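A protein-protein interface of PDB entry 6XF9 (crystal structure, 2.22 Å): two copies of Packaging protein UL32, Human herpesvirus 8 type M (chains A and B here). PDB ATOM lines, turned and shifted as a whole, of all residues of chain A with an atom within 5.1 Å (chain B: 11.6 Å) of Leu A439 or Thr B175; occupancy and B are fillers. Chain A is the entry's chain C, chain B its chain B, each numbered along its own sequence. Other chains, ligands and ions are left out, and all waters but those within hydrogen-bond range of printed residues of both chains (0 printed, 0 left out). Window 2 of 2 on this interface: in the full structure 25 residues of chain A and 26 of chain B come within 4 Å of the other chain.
Of the 19 printed residues of chain B, 3 touch a printed residue of chain A.
Printed residues of chain B that touch a printed residue of chain A: Asn B150, Thr B175 and Ser B176.
Hydrophobic or aromatic side chains of chain A that line the printed part of chain B: Leu A439, Ile A442 and His A458.
Among the printed residues, no Asp or Glu carboxylate lies within 4 Å of a Lys or Arg side-chain nitrogen of the other chain.
A ring nitrogen (ND1) of His A458 lies within hydrogen-bond range of the side-chain hydroxyl (OG) of Ser A460 (2.8 Å).
Positions printed for both chains: 436, 437, 438, 440 and 441.
The side-chain amide oxygen (OD1) of Asn B150 lies within hydrogen-bond range of the backbone NH (N) of His A458, 3.2 Å away.
OG of Ser B176 lies within hydrogen-bond range of OG of Ser A460, at 2.9 Å.
Thr B175 touches four residues of chain A.
No residue of chain B comes within 4 Å of Lys A435.
No residue of chain B comes within 4 Å of Thr A436.
No residue of chain B comes within 4 Å of Thr A437.
No residue of chain B comes within 4 Å of Ser A438.
No residue of chain B comes within 4 Å of Ile A441.
Ile A442 touches just one residue of chain B: Thr B175 (3.7 Å).
No residue of chain B comes within 4 Å of Arg A443.
Ser A460 touches just these residues of chain B: Thr B175 and Ser B176.
Of the printed residues of chain A, Ser B176 touches Ser A460.
Printed residues of chain A within 4 Å of Asn B150: His A458 (3.2 Å).
The nearest residue of chain B that does not touch Leu A439 is Lys B174 (6.7 Å).
The nearest printed residue of chain A that does not touch Thr B175 is Arg A443 (5.3 Å).
Among the printed residues, merely in contact across the chains: Leu A439 with Thr B175, Ile A442 with Thr B175, His A458 with Thr B175 and Ser A460 with Thr B175.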
ATOM      1  N   LYS A 435     -26.728 -31.598 -19.343  1.00  0.00           N
ATOM      2  CA  LYS A 435     -25.895 -30.959 -20.361  1.00  0.00           C
ATOM      3  C   LYS A 435     -24.443 -31.421 -20.280  1.00  0.00           C
ATOM      4  O   LYS A 435     -23.756 -31.525 -21.312  1.00  0.00           O
ATOM      5  CB  LYS A 435     -26.006 -29.434 -20.280  1.00  0.00           C
ATOM      6  CG  LYS A 435     -25.434 -28.738 -21.536  1.00  0.00           C
ATOM      7  CD  LYS A 435     -26.181 -29.083 -22.848  1.00  0.00           C
ATOM      8  CE  LYS A 435     -25.501 -28.403 -24.047  1.00  0.00           C
ATOM      9  NZ  LYS A 435     -26.204 -28.609 -25.344  1.00  0.00           N
ATOM     10  N   THR A 436     -23.960 -31.759 -19.088  1.00  0.00           N
ATOM     11  CA  THR A 436     -22.593 -32.253 -19.027  1.00  0.00           C
ATOM     12  C   THR A 436     -22.493 -33.639 -19.637  1.00  0.00           C
ATOM     13  O   THR A 436     -21.574 -33.903 -20.422  1.00  0.00           O
ATOM     14  CB  THR A 436     -22.080 -32.284 -17.593  1.00  0.00           C
ATOM     15  OG1 THR A 436     -22.086 -30.963 -17.044  1.00  0.00           O
ATOM     16  CG2 THR A 436     -20.671 -32.849 -17.559  1.00  0.00           C
ATOM     17  N   THR A 437     -23.468 -34.519 -19.368  1.00  0.00           N
ATOM     18  CA  THR A 437     -23.363 -35.823 -20.001  1.00  0.00           C
ATOM     19  C   THR A 437     -23.538 -35.687 -21.505  1.00  0.00           C
ATOM     20  O   THR A 437     -22.909 -36.437 -22.261  1.00  0.00           O
ATOM     21  CB  THR A 437     -24.367 -36.829 -19.400  1.00  0.00           C
ATOM     22  OG1 THR A 437     -25.695 -36.457 -19.741  1.00  0.00           O
ATOM     23  CG2 THR A 437     -24.266 -36.916 -17.859  1.00  0.00           C
ATOM     24  N   SER A 438     -24.259 -34.648 -21.959  1.00  0.00           N
ATOM     25  CA  SER A 438     -24.399 -34.411 -23.399  1.00  0.00           C
ATOM     26  C   SER A 438     -23.068 -34.042 -24.040  1.00  0.00           C
ATOM     27  O   SER A 438     -22.673 -34.626 -25.061  1.00  0.00           O
ATOM     28  CB  SER A 438     -25.423 -33.314 -23.678  1.00  0.00           C
ATOM     29  OG  SER A 438     -26.761 -33.781 -23.546  1.00  0.00           O
ATOM     30  N   LEU A 439     -22.333 -33.110 -23.442  1.00  0.00           N
ATOM     31  CA  LEU A 439     -21.093 -32.752 -24.112  1.00  0.00           C
ATOM     32  C   LEU A 439     -19.995 -33.777 -23.863  1.00  0.00           C
ATOM     33  O   LEU A 439     -19.061 -33.872 -24.672  1.00  0.00           O
ATOM     34  CB  LEU A 439     -20.673 -31.334 -23.724  1.00  0.00           C
ATOM     35  CG  LEU A 439     -21.803 -30.303 -24.014  1.00  0.00           C
ATOM     36  CD1 LEU A 439     -21.424 -28.900 -23.626  1.00  0.00           C
ATOM     37  CD2 LEU A 439     -22.408 -30.273 -25.438  1.00  0.00           C
ATOM     38  N   ASP A 440     -20.147 -34.628 -22.838  1.00  0.00           N
ATOM     39  CA  ASP A 440     -19.191 -35.717 -22.629  1.00  0.00           C
ATOM     40  C   ASP A 440     -19.334 -36.761 -23.737  1.00  0.00           C
ATOM     41  O   ASP A 440     -18.338 -37.237 -24.320  1.00  0.00           O
ATOM     42  CB  ASP A 440     -19.447 -36.386 -21.273  1.00  0.00           C
ATOM     43  CG  ASP A 440     -19.290 -35.435 -20.094  1.00  0.00           C
ATOM     44  OD1 ASP A 440     -18.418 -34.537 -20.123  1.00  0.00           O
ATOM     45  OD2 ASP A 440     -20.059 -35.605 -19.114  1.00  0.00           O
ATOM     46  N   ILE A 441     -20.591 -37.124 -24.033  1.00  0.00           N
ATOM     47  CA  ILE A 441     -20.879 -38.031 -25.138  1.00  0.00           C
ATOM     48  C   ILE A 441     -20.363 -37.443 -26.444  1.00  0.00           C
ATOM     49  O   ILE A 441     -19.742 -38.138 -27.253  1.00  0.00           O
ATOM     50  CB  ILE A 441     -22.387 -38.303 -25.234  1.00  0.00           C
ATOM     51  CG1 ILE A 441     -22.938 -38.980 -23.984  1.00  0.00           C
ATOM     52  CG2 ILE A 441     -22.634 -39.210 -26.396  1.00  0.00           C
ATOM     53  CD1 ILE A 441     -24.457 -39.029 -23.976  1.00  0.00           C
ATOM     54  N   ILE A 442     -20.652 -36.157 -26.685  1.00  0.00           N
ATOM     55  CA  ILE A 442     -20.224 -35.529 -27.934  1.00  0.00           C
ATOM     56  C   ILE A 442     -18.719 -35.613 -28.086  1.00  0.00           C
ATOM     57  O   ILE A 442     -18.195 -35.893 -29.177  1.00  0.00           O
ATOM     58  CB  ILE A 442     -20.704 -34.072 -27.991  1.00  0.00           C
ATOM     59  CG1 ILE A 442     -22.187 -34.020 -28.344  1.00  0.00           C
ATOM     60  CG2 ILE A 442     -19.858 -33.274 -28.959  1.00  0.00           C
ATOM     61  CD1 ILE A 442     -22.773 -32.650 -28.142  1.00  0.00           C
ATOM     62  N   ARG A 443     -17.989 -35.392 -27.001  1.00  0.00           N
ATOM     63  CA  ARG A 443     -16.544 -35.402 -27.166  1.00  0.00           C
ATOM     64  C   ARG A 443     -16.036 -36.789 -27.499  1.00  0.00           C
ATOM     65  O   ARG A 443     -15.205 -36.950 -28.409  1.00  0.00           O
ATOM     66  CB  ARG A 443     -15.857 -34.889 -25.926  1.00  0.00           C
ATOM     67  CG  ARG A 443     -14.413 -34.716 -26.216  1.00  0.00           C
ATOM     68  CD  ARG A 443     -13.734 -34.145 -25.017  1.00  0.00           C
ATOM     69  NE  ARG A 443     -14.283 -32.832 -24.684  1.00  0.00           N
ATOM     70  CZ  ARG A 443     -13.864 -31.665 -25.181  1.00  0.00           C
ATOM     71  NH1 ARG A 443     -12.870 -31.595 -26.072  1.00  0.00           N
ATOM     72  NH2 ARG A 443     -14.460 -30.550 -24.782  1.00  0.00           N
ATOM     73  N   HIS A 458     -19.246 -31.703 -37.326  1.00  0.00           N
ATOM     74  CA  HIS A 458     -19.019 -31.880 -35.904  1.00  0.00           C
ATOM     75  C   HIS A 458     -20.333 -32.231 -35.214  1.00  0.00           C
ATOM     76  O   HIS A 458     -21.353 -31.579 -35.475  1.00  0.00           O
ATOM     77  CB  HIS A 458     -18.417 -30.643 -35.273  1.00  0.00           C
ATOM     78  CG  HIS A 458     -17.880 -30.911 -33.909  1.00  0.00           C
ATOM     79  ND1 HIS A 458     -18.655 -30.810 -32.775  1.00  0.00           N
ATOM     80  CD2 HIS A 458     -16.674 -31.375 -33.504  1.00  0.00           C
ATOM     81  CE1 HIS A 458     -17.932 -31.150 -31.722  1.00  0.00           C
ATOM     82  NE2 HIS A 458     -16.729 -31.501 -32.138  1.00  0.00           N
ATOM     83  N   SER A 460     -21.696 -31.534 -32.435  1.00  0.00           N
ATOM     84  CA  SER A 460     -22.462 -30.437 -31.825  1.00  0.00           C
ATOM     85  C   SER A 460     -23.236 -29.634 -32.876  1.00  0.00           C
ATOM     86  O   SER A 460     -24.385 -29.222 -32.638  1.00  0.00           O
ATOM     87  CB  SER A 460     -21.559 -29.536 -30.997  1.00  0.00           C
ATOM     88  OG  SER A 460     -20.496 -29.023 -31.760  1.00  0.00           O
ATOM     89  N   ASN B 150     -17.890 -26.282 -40.394  1.00  0.00           N
ATOM     90  CA  ASN B 150     -17.916 -26.041 -38.950  1.00  0.00           C
ATOM     91  C   ASN B 150     -17.692 -24.565 -38.656  1.00  0.00           C
ATOM     92  O   ASN B 150     -18.517 -23.917 -37.992  1.00  0.00           O
ATOM     93  CB  ASN B 150     -16.880 -26.916 -38.256  1.00  0.00           C
ATOM     94  CG  ASN B 150     -17.196 -28.394 -38.436  1.00  0.00           C
ATOM     95  OD1 ASN B 150     -18.377 -28.821 -38.368  1.00  0.00           O
ATOM     96  ND2 ASN B 150     -16.161 -29.183 -38.747  1.00  0.00           N
ATOM     97  N   LEU B 151     -16.643 -23.989 -39.253  1.00  0.00           N
ATOM     98  CA  LEU B 151     -16.341 -22.583 -39.014  1.00  0.00           C
ATOM     99  C   LEU B 151     -17.471 -21.693 -39.504  1.00  0.00           C
ATOM    100  O   LEU B 151     -17.880 -20.762 -38.803  1.00  0.00           O
ATOM    101  CB  LEU B 151     -15.024 -22.230 -39.694  1.00  0.00           C
ATOM    102  CG  LEU B 151     -13.773 -22.820 -39.060  1.00  0.00           C
ATOM    103  CD1 LEU B 151     -12.582 -22.413 -39.855  1.00  0.00           C
ATOM    104  CD2 LEU B 151     -13.638 -22.215 -37.712  1.00  0.00           C
ATOM    105  N   PHE B 153     -20.599 -22.448 -39.596  1.00  0.00           N
ATOM    106  CA  PHE B 153     -21.630 -22.598 -38.580  1.00  0.00           C
ATOM    107  C   PHE B 153     -21.436 -21.560 -37.488  1.00  0.00           C
ATOM    108  O   PHE B 153     -22.320 -20.730 -37.230  1.00  0.00           O
ATOM    109  CB  PHE B 153     -21.568 -24.017 -38.016  1.00  0.00           C
ATOM    110  CG  PHE B 153     -22.599 -24.299 -36.970  1.00  0.00           C
ATOM    111  CD1 PHE B 153     -23.915 -24.536 -37.328  1.00  0.00           C
ATOM    112  CD2 PHE B 153     -22.247 -24.333 -35.621  1.00  0.00           C
ATOM    113  CE1 PHE B 153     -24.864 -24.793 -36.363  1.00  0.00           C
ATOM    114  CE2 PHE B 153     -23.187 -24.587 -34.649  1.00  0.00           C
ATOM    115  CZ  PHE B 153     -24.495 -24.818 -35.010  1.00  0.00           C
ATOM    116  N   LEU B 154     -20.235 -21.537 -36.894  1.00  0.00           N
ATOM    117  CA  LEU B 154     -19.979 -20.602 -35.805  1.00  0.00           C
ATOM    118  C   LEU B 154     -20.215 -19.170 -36.255  1.00  0.00           C
ATOM    119  O   LEU B 154     -20.889 -18.394 -35.557  1.00  0.00           O
ATOM    120  CB  LEU B 154     -18.557 -20.768 -35.304  1.00  0.00           C
ATOM    121  CG  LEU B 154     -18.239 -22.099 -34.641  1.00  0.00           C
ATOM    122  CD1 LEU B 154     -16.779 -22.115 -34.206  1.00  0.00           C
ATOM    123  CD2 LEU B 154     -19.166 -22.346 -33.474  1.00  0.00           C
ATOM    124  N   GLU B 157     -23.870 -18.264 -36.322  1.00  0.00           N
ATOM    125  CA  GLU B 157     -24.486 -18.132 -35.009  1.00  0.00           C
ATOM    126  C   GLU B 157     -24.183 -16.761 -34.442  1.00  0.00           C
ATOM    127  O   GLU B 157     -25.100 -15.978 -34.152  1.00  0.00           O
ATOM    128  CB  GLU B 157     -24.009 -19.240 -34.068  1.00  0.00           C
ATOM    129  CG  GLU B 157     -24.494 -20.648 -34.445  1.00  0.00           C
ATOM    130  CD  GLU B 157     -26.011 -20.806 -34.286  1.00  0.00           C
ATOM    131  OE1 GLU B 157     -26.726 -21.022 -35.311  1.00  0.00           O
ATOM    132  OE2 GLU B 157     -26.479 -20.717 -33.118  1.00  0.00           O
ATOM    133  N   PHE B 158     -22.910 -16.379 -34.444  1.00  0.00           N
ATOM    134  CA  PHE B 158     -22.620 -15.147 -33.742  1.00  0.00           C
ATOM    135  C   PHE B 158     -23.102 -13.945 -34.525  1.00  0.00           C
ATOM    136  O   PHE B 158     -23.562 -12.974 -33.921  1.00  0.00           O
ATOM    137  CB  PHE B 158     -21.148 -15.089 -33.411  1.00  0.00           C
ATOM    138  CG  PHE B 158     -20.786 -15.942 -32.232  1.00  0.00           C
ATOM    139  CD1 PHE B 158     -20.847 -17.332 -32.325  1.00  0.00           C
ATOM    140  CD2 PHE B 158     -20.425 -15.362 -31.016  1.00  0.00           C
ATOM    141  CE1 PHE B 158     -20.534 -18.135 -31.223  1.00  0.00           C
ATOM    142  CE2 PHE B 158     -20.091 -16.154 -29.917  1.00  0.00           C
ATOM    143  CZ  PHE B 158     -20.147 -17.544 -30.025  1.00  0.00           C
ATOM    144  N   THR B 168     -27.362 -18.223 -28.709  1.00  0.00           N
ATOM    145  CA  THR B 168     -27.729 -19.499 -28.108  1.00  0.00           C
ATOM    146  C   THR B 168     -26.548 -20.464 -28.098  1.00  0.00           C
ATOM    147  O   THR B 168     -26.044 -20.854 -29.151  1.00  0.00           O
ATOM    148  CB  THR B 168     -28.908 -20.154 -28.850  1.00  0.00           C
ATOM    149  OG1 THR B 168     -29.232 -21.404 -28.231  1.00  0.00           O
ATOM    150  CG2 THR B 168     -28.552 -20.393 -30.310  1.00  0.00           C
ATOM    151  N   PHE B 173     -19.560 -22.989 -28.771  1.00  0.00           N
ATOM    152  CA  PHE B 173     -18.164 -22.697 -29.108  1.00  0.00           C
ATOM    153  C   PHE B 173     -17.132 -23.702 -28.556  1.00  0.00           C
ATOM    154  O   PHE B 173     -16.373 -24.306 -29.329  1.00  0.00           O
ATOM    155  CB  PHE B 173     -17.778 -21.306 -28.599  1.00  0.00           C
ATOM    156  CG  PHE B 173     -16.300 -21.013 -28.718  1.00  0.00           C
ATOM    157  CD1 PHE B 173     -15.743 -20.689 -29.946  1.00  0.00           C
ATOM    158  CD2 PHE B 173     -15.464 -21.089 -27.611  1.00  0.00           C
ATOM    159  CE1 PHE B 173     -14.385 -20.423 -30.074  1.00  0.00           C
ATOM    160  CE2 PHE B 173     -14.099 -20.832 -27.731  1.00  0.00           C
ATOM    161  CZ  PHE B 173     -13.559 -20.498 -28.965  1.00  0.00           C
ATOM    162  N   LYS B 174     -17.097 -23.852 -27.221  1.00  0.00           N
ATOM    163  CA  LYS B 174     -16.153 -24.768 -26.580  1.00  0.00           C
ATOM    164  C   LYS B 174     -16.345 -26.194 -27.080  1.00  0.00           C
ATOM    165  O   LYS B 174     -15.379 -26.958 -27.203  1.00  0.00           O
ATOM    166  CB  LYS B 174     -16.311 -24.710 -25.061  1.00  0.00           C
ATOM    167  N   THR B 175     -17.595 -26.588 -27.337  1.00  0.00           N
ATOM    168  CA  THR B 175     -17.827 -27.905 -27.912  1.00  0.00           C
ATOM    169  C   THR B 175     -17.237 -27.987 -29.317  1.00  0.00           C
ATOM    170  O   THR B 175     -16.493 -28.923 -29.628  1.00  0.00           O
ATOM    171  CB  THR B 175     -19.329 -28.209 -27.960  1.00  0.00           C
ATOM    172  OG1 THR B 175     -19.902 -28.075 -26.653  1.00  0.00           O
ATOM    173  CG2 THR B 175     -19.523 -29.641 -28.386  1.00  0.00           C
ATOM    174  N   SER B 176     -17.505 -26.969 -30.169  1.00  0.00           N
ATOM    175  CA  SER B 176     -17.223 -27.087 -31.606  1.00  0.00           C
ATOM    176  C   SER B 176     -15.780 -26.756 -31.967  1.00  0.00           C
ATOM    177  O   SER B 176     -15.296 -27.236 -32.997  1.00  0.00           O
ATOM    178  CB  SER B 176     -18.116 -26.150 -32.449  1.00  0.00           C
ATOM    179  OG  SER B 176     -19.507 -26.279 -32.198  1.00  0.00           O
ATOM    180  N   TRP B 177     -15.066 -26.006 -31.128  1.00  0.00           N
ATOM    181  CA  TRP B 177     -13.757 -25.495 -31.517  1.00  0.00           C
ATOM    182  C   TRP B 177     -12.711 -26.591 -31.441  1.00  0.00           C
ATOM    183  O   TRP B 177     -12.189 -26.858 -30.359  1.00  0.00           O
ATOM    184  CB  TRP B 177     -13.339 -24.336 -30.624  1.00  0.00           C
ATOM    185  CG  TRP B 177     -12.198 -23.556 -31.200  1.00  0.00           C
ATOM    186  CD1 TRP B 177     -10.890 -23.575 -30.789  1.00  0.00           C
ATOM    187  CD2 TRP B 177     -12.268 -22.604 -32.271  1.00  0.00           C
ATOM    188  NE1 TRP B 177     -10.135 -22.715 -31.562  1.00  0.00           N
ATOM    189  CE2 TRP B 177     -10.958 -22.108 -32.479  1.00  0.00           C
ATOM    190  CE3 TRP B 177     -13.305 -22.138 -33.090  1.00  0.00           C
ATOM    191  CZ2 TRP B 177     -10.666 -21.164 -33.468  1.00  0.00           C
ATOM    192  CZ3 TRP B 177     -13.008 -21.209 -34.081  1.00  0.00           C
ATOM    193  CH2 TRP B 177     -11.704 -20.729 -34.254  1.00  0.00           C
ATOM    194  N   LEU B 424     -16.722 -13.870 -33.837  1.00  0.00           N
ATOM    195  CA  LEU B 424     -17.111 -14.227 -32.480  1.00  0.00           C
ATOM    196  C   LEU B 424     -16.867 -13.068 -31.524  1.00  0.00           C
ATOM    197  O   LEU B 424     -17.742 -12.724 -30.725  1.00  0.00           O
ATOM    198  CB  LEU B 424     -16.352 -15.479 -32.042  1.00  0.00           C
ATOM    199  CG  LEU B 424     -17.113 -16.789 -32.307  1.00  0.00           C
ATOM    200  CD1 LEU B 424     -17.692 -16.863 -33.727  1.00  0.00           C
ATOM    201  CD2 LEU B 424     -16.257 -18.021 -31.994  1.00  0.00           C
ATOM    202  N   THR B 436     -18.428 -17.102 -19.434  1.00  0.00           N
ATOM    203  CA  THR B 436     -17.298 -17.988 -19.667  1.00  0.00           C
ATOM    204  C   THR B 436     -17.044 -18.185 -21.162  1.00  0.00           C
ATOM    205  O   THR B 436     -15.880 -18.253 -21.572  1.00  0.00           O
ATOM    206  CB  THR B 436     -17.451 -19.330 -18.928  1.00  0.00           C
ATOM    207  OG1 THR B 436     -17.526 -19.115 -17.519  1.00  0.00           O
ATOM    208  CG2 THR B 436     -16.295 -20.280 -19.246  1.00  0.00           C
ATOM    209  N   THR B 437     -18.082 -18.273 -22.014  1.00  0.00           N
ATOM    210  CA  THR B 437     -17.741 -18.394 -23.438  1.00  0.00           C
ATOM    211  C   THR B 437     -17.126 -17.091 -23.955  1.00  0.00           C
ATOM    212  O   THR B 437     -16.312 -17.117 -24.888  1.00  0.00           O
ATOM    213  CB  THR B 437     -18.941 -18.810 -24.303  1.00  0.00           C
ATOM    214  OG1 THR B 437     -19.859 -17.733 -24.432  1.00  0.00           O
ATOM    215  CG2 THR B 437     -19.688 -19.959 -23.654  1.00  0.00           C
ATOM    216  N   SER B 438     -17.435 -15.956 -23.314  1.00  0.00           N
ATOM    217  CA  SER B 438     -16.732 -14.718 -23.651  1.00  0.00           C
ATOM    218  C   SER B 438     -15.255 -14.805 -23.293  1.00  0.00           C
ATOM    219  O   SER B 438     -14.394 -14.458 -24.113  1.00  0.00           O
ATOM    220  CB  SER B 438     -17.349 -13.520 -22.936  1.00  0.00           C
ATOM    221  OG  SER B 438     -18.543 -13.111 -23.569  1.00  0.00           O
ATOM    222  N   ASP B 440     -13.519 -17.429 -23.035  1.00  0.00           N
ATOM    223  CA  ASP B 440     -12.877 -18.454 -23.850  1.00  0.00           C
ATOM    224  C   ASP B 440     -12.527 -17.909 -25.220  1.00  0.00           C
ATOM    225  O   ASP B 440     -11.416 -18.123 -25.732  1.00  0.00           O
ATOM    226  CB  ASP B 440     -13.785 -19.671 -23.998  1.00  0.00           C
ATOM    227  CG  ASP B 440     -13.977 -20.412 -22.695  1.00  0.00           C
ATOM    228  OD1 ASP B 440     -13.022 -20.448 -21.874  1.00  0.00           O
ATOM    229  OD2 ASP B 440     -15.067 -21.020 -22.525  1.00  0.00           O
ATOM    230  N   ILE B 441     -13.480 -17.205 -25.835  1.00  0.00           N
ATOM    231  CA  ILE B 441     -13.212 -16.543 -27.103  1.00  0.00           C
ATOM    232  C   ILE B 441     -12.042 -15.579 -26.954  1.00  0.00           C
ATOM    233  O   ILE B 441     -11.150 -15.539 -27.801  1.00  0.00           O
ATOM    234  CB  ILE B 441     -14.474 -15.833 -27.618  1.00  0.00           C
ATOM    235  CG1 ILE B 441     -15.563 -16.853 -27.949  1.00  0.00           C
ATOM    236  CG2 ILE B 441     -14.139 -14.998 -28.836  1.00  0.00           C
ATOM    237  CD1 ILE B 441     -16.880 -16.213 -28.288  1.00  0.00           C
ATOM    238  N   GLU B 444      -8.681 -17.472 -26.764  1.00  0.00           N
ATOM    239  CA  GLU B 444      -8.308 -18.067 -28.045  1.00  0.00           C
ATOM    240  C   GLU B 444      -7.930 -16.991 -29.055  1.00  0.00           C
ATOM    241  O   GLU B 444      -6.958 -17.138 -29.804  1.00  0.00           O
ATOM    242  CB  GLU B 444      -9.461 -18.910 -28.582  1.00  0.00           C
ATOM    243  CG  GLU B 444      -9.076 -19.679 -29.797  1.00  0.00           C
ATOM    244  CD  GLU B 444      -7.963 -20.651 -29.480  1.00  0.00           C
ATOM    245  OE1 GLU B 444      -7.880 -21.055 -28.293  1.00  0.00           O
ATOM    246  OE2 GLU B 444      -7.146 -20.980 -30.381  1.00  0.00           O
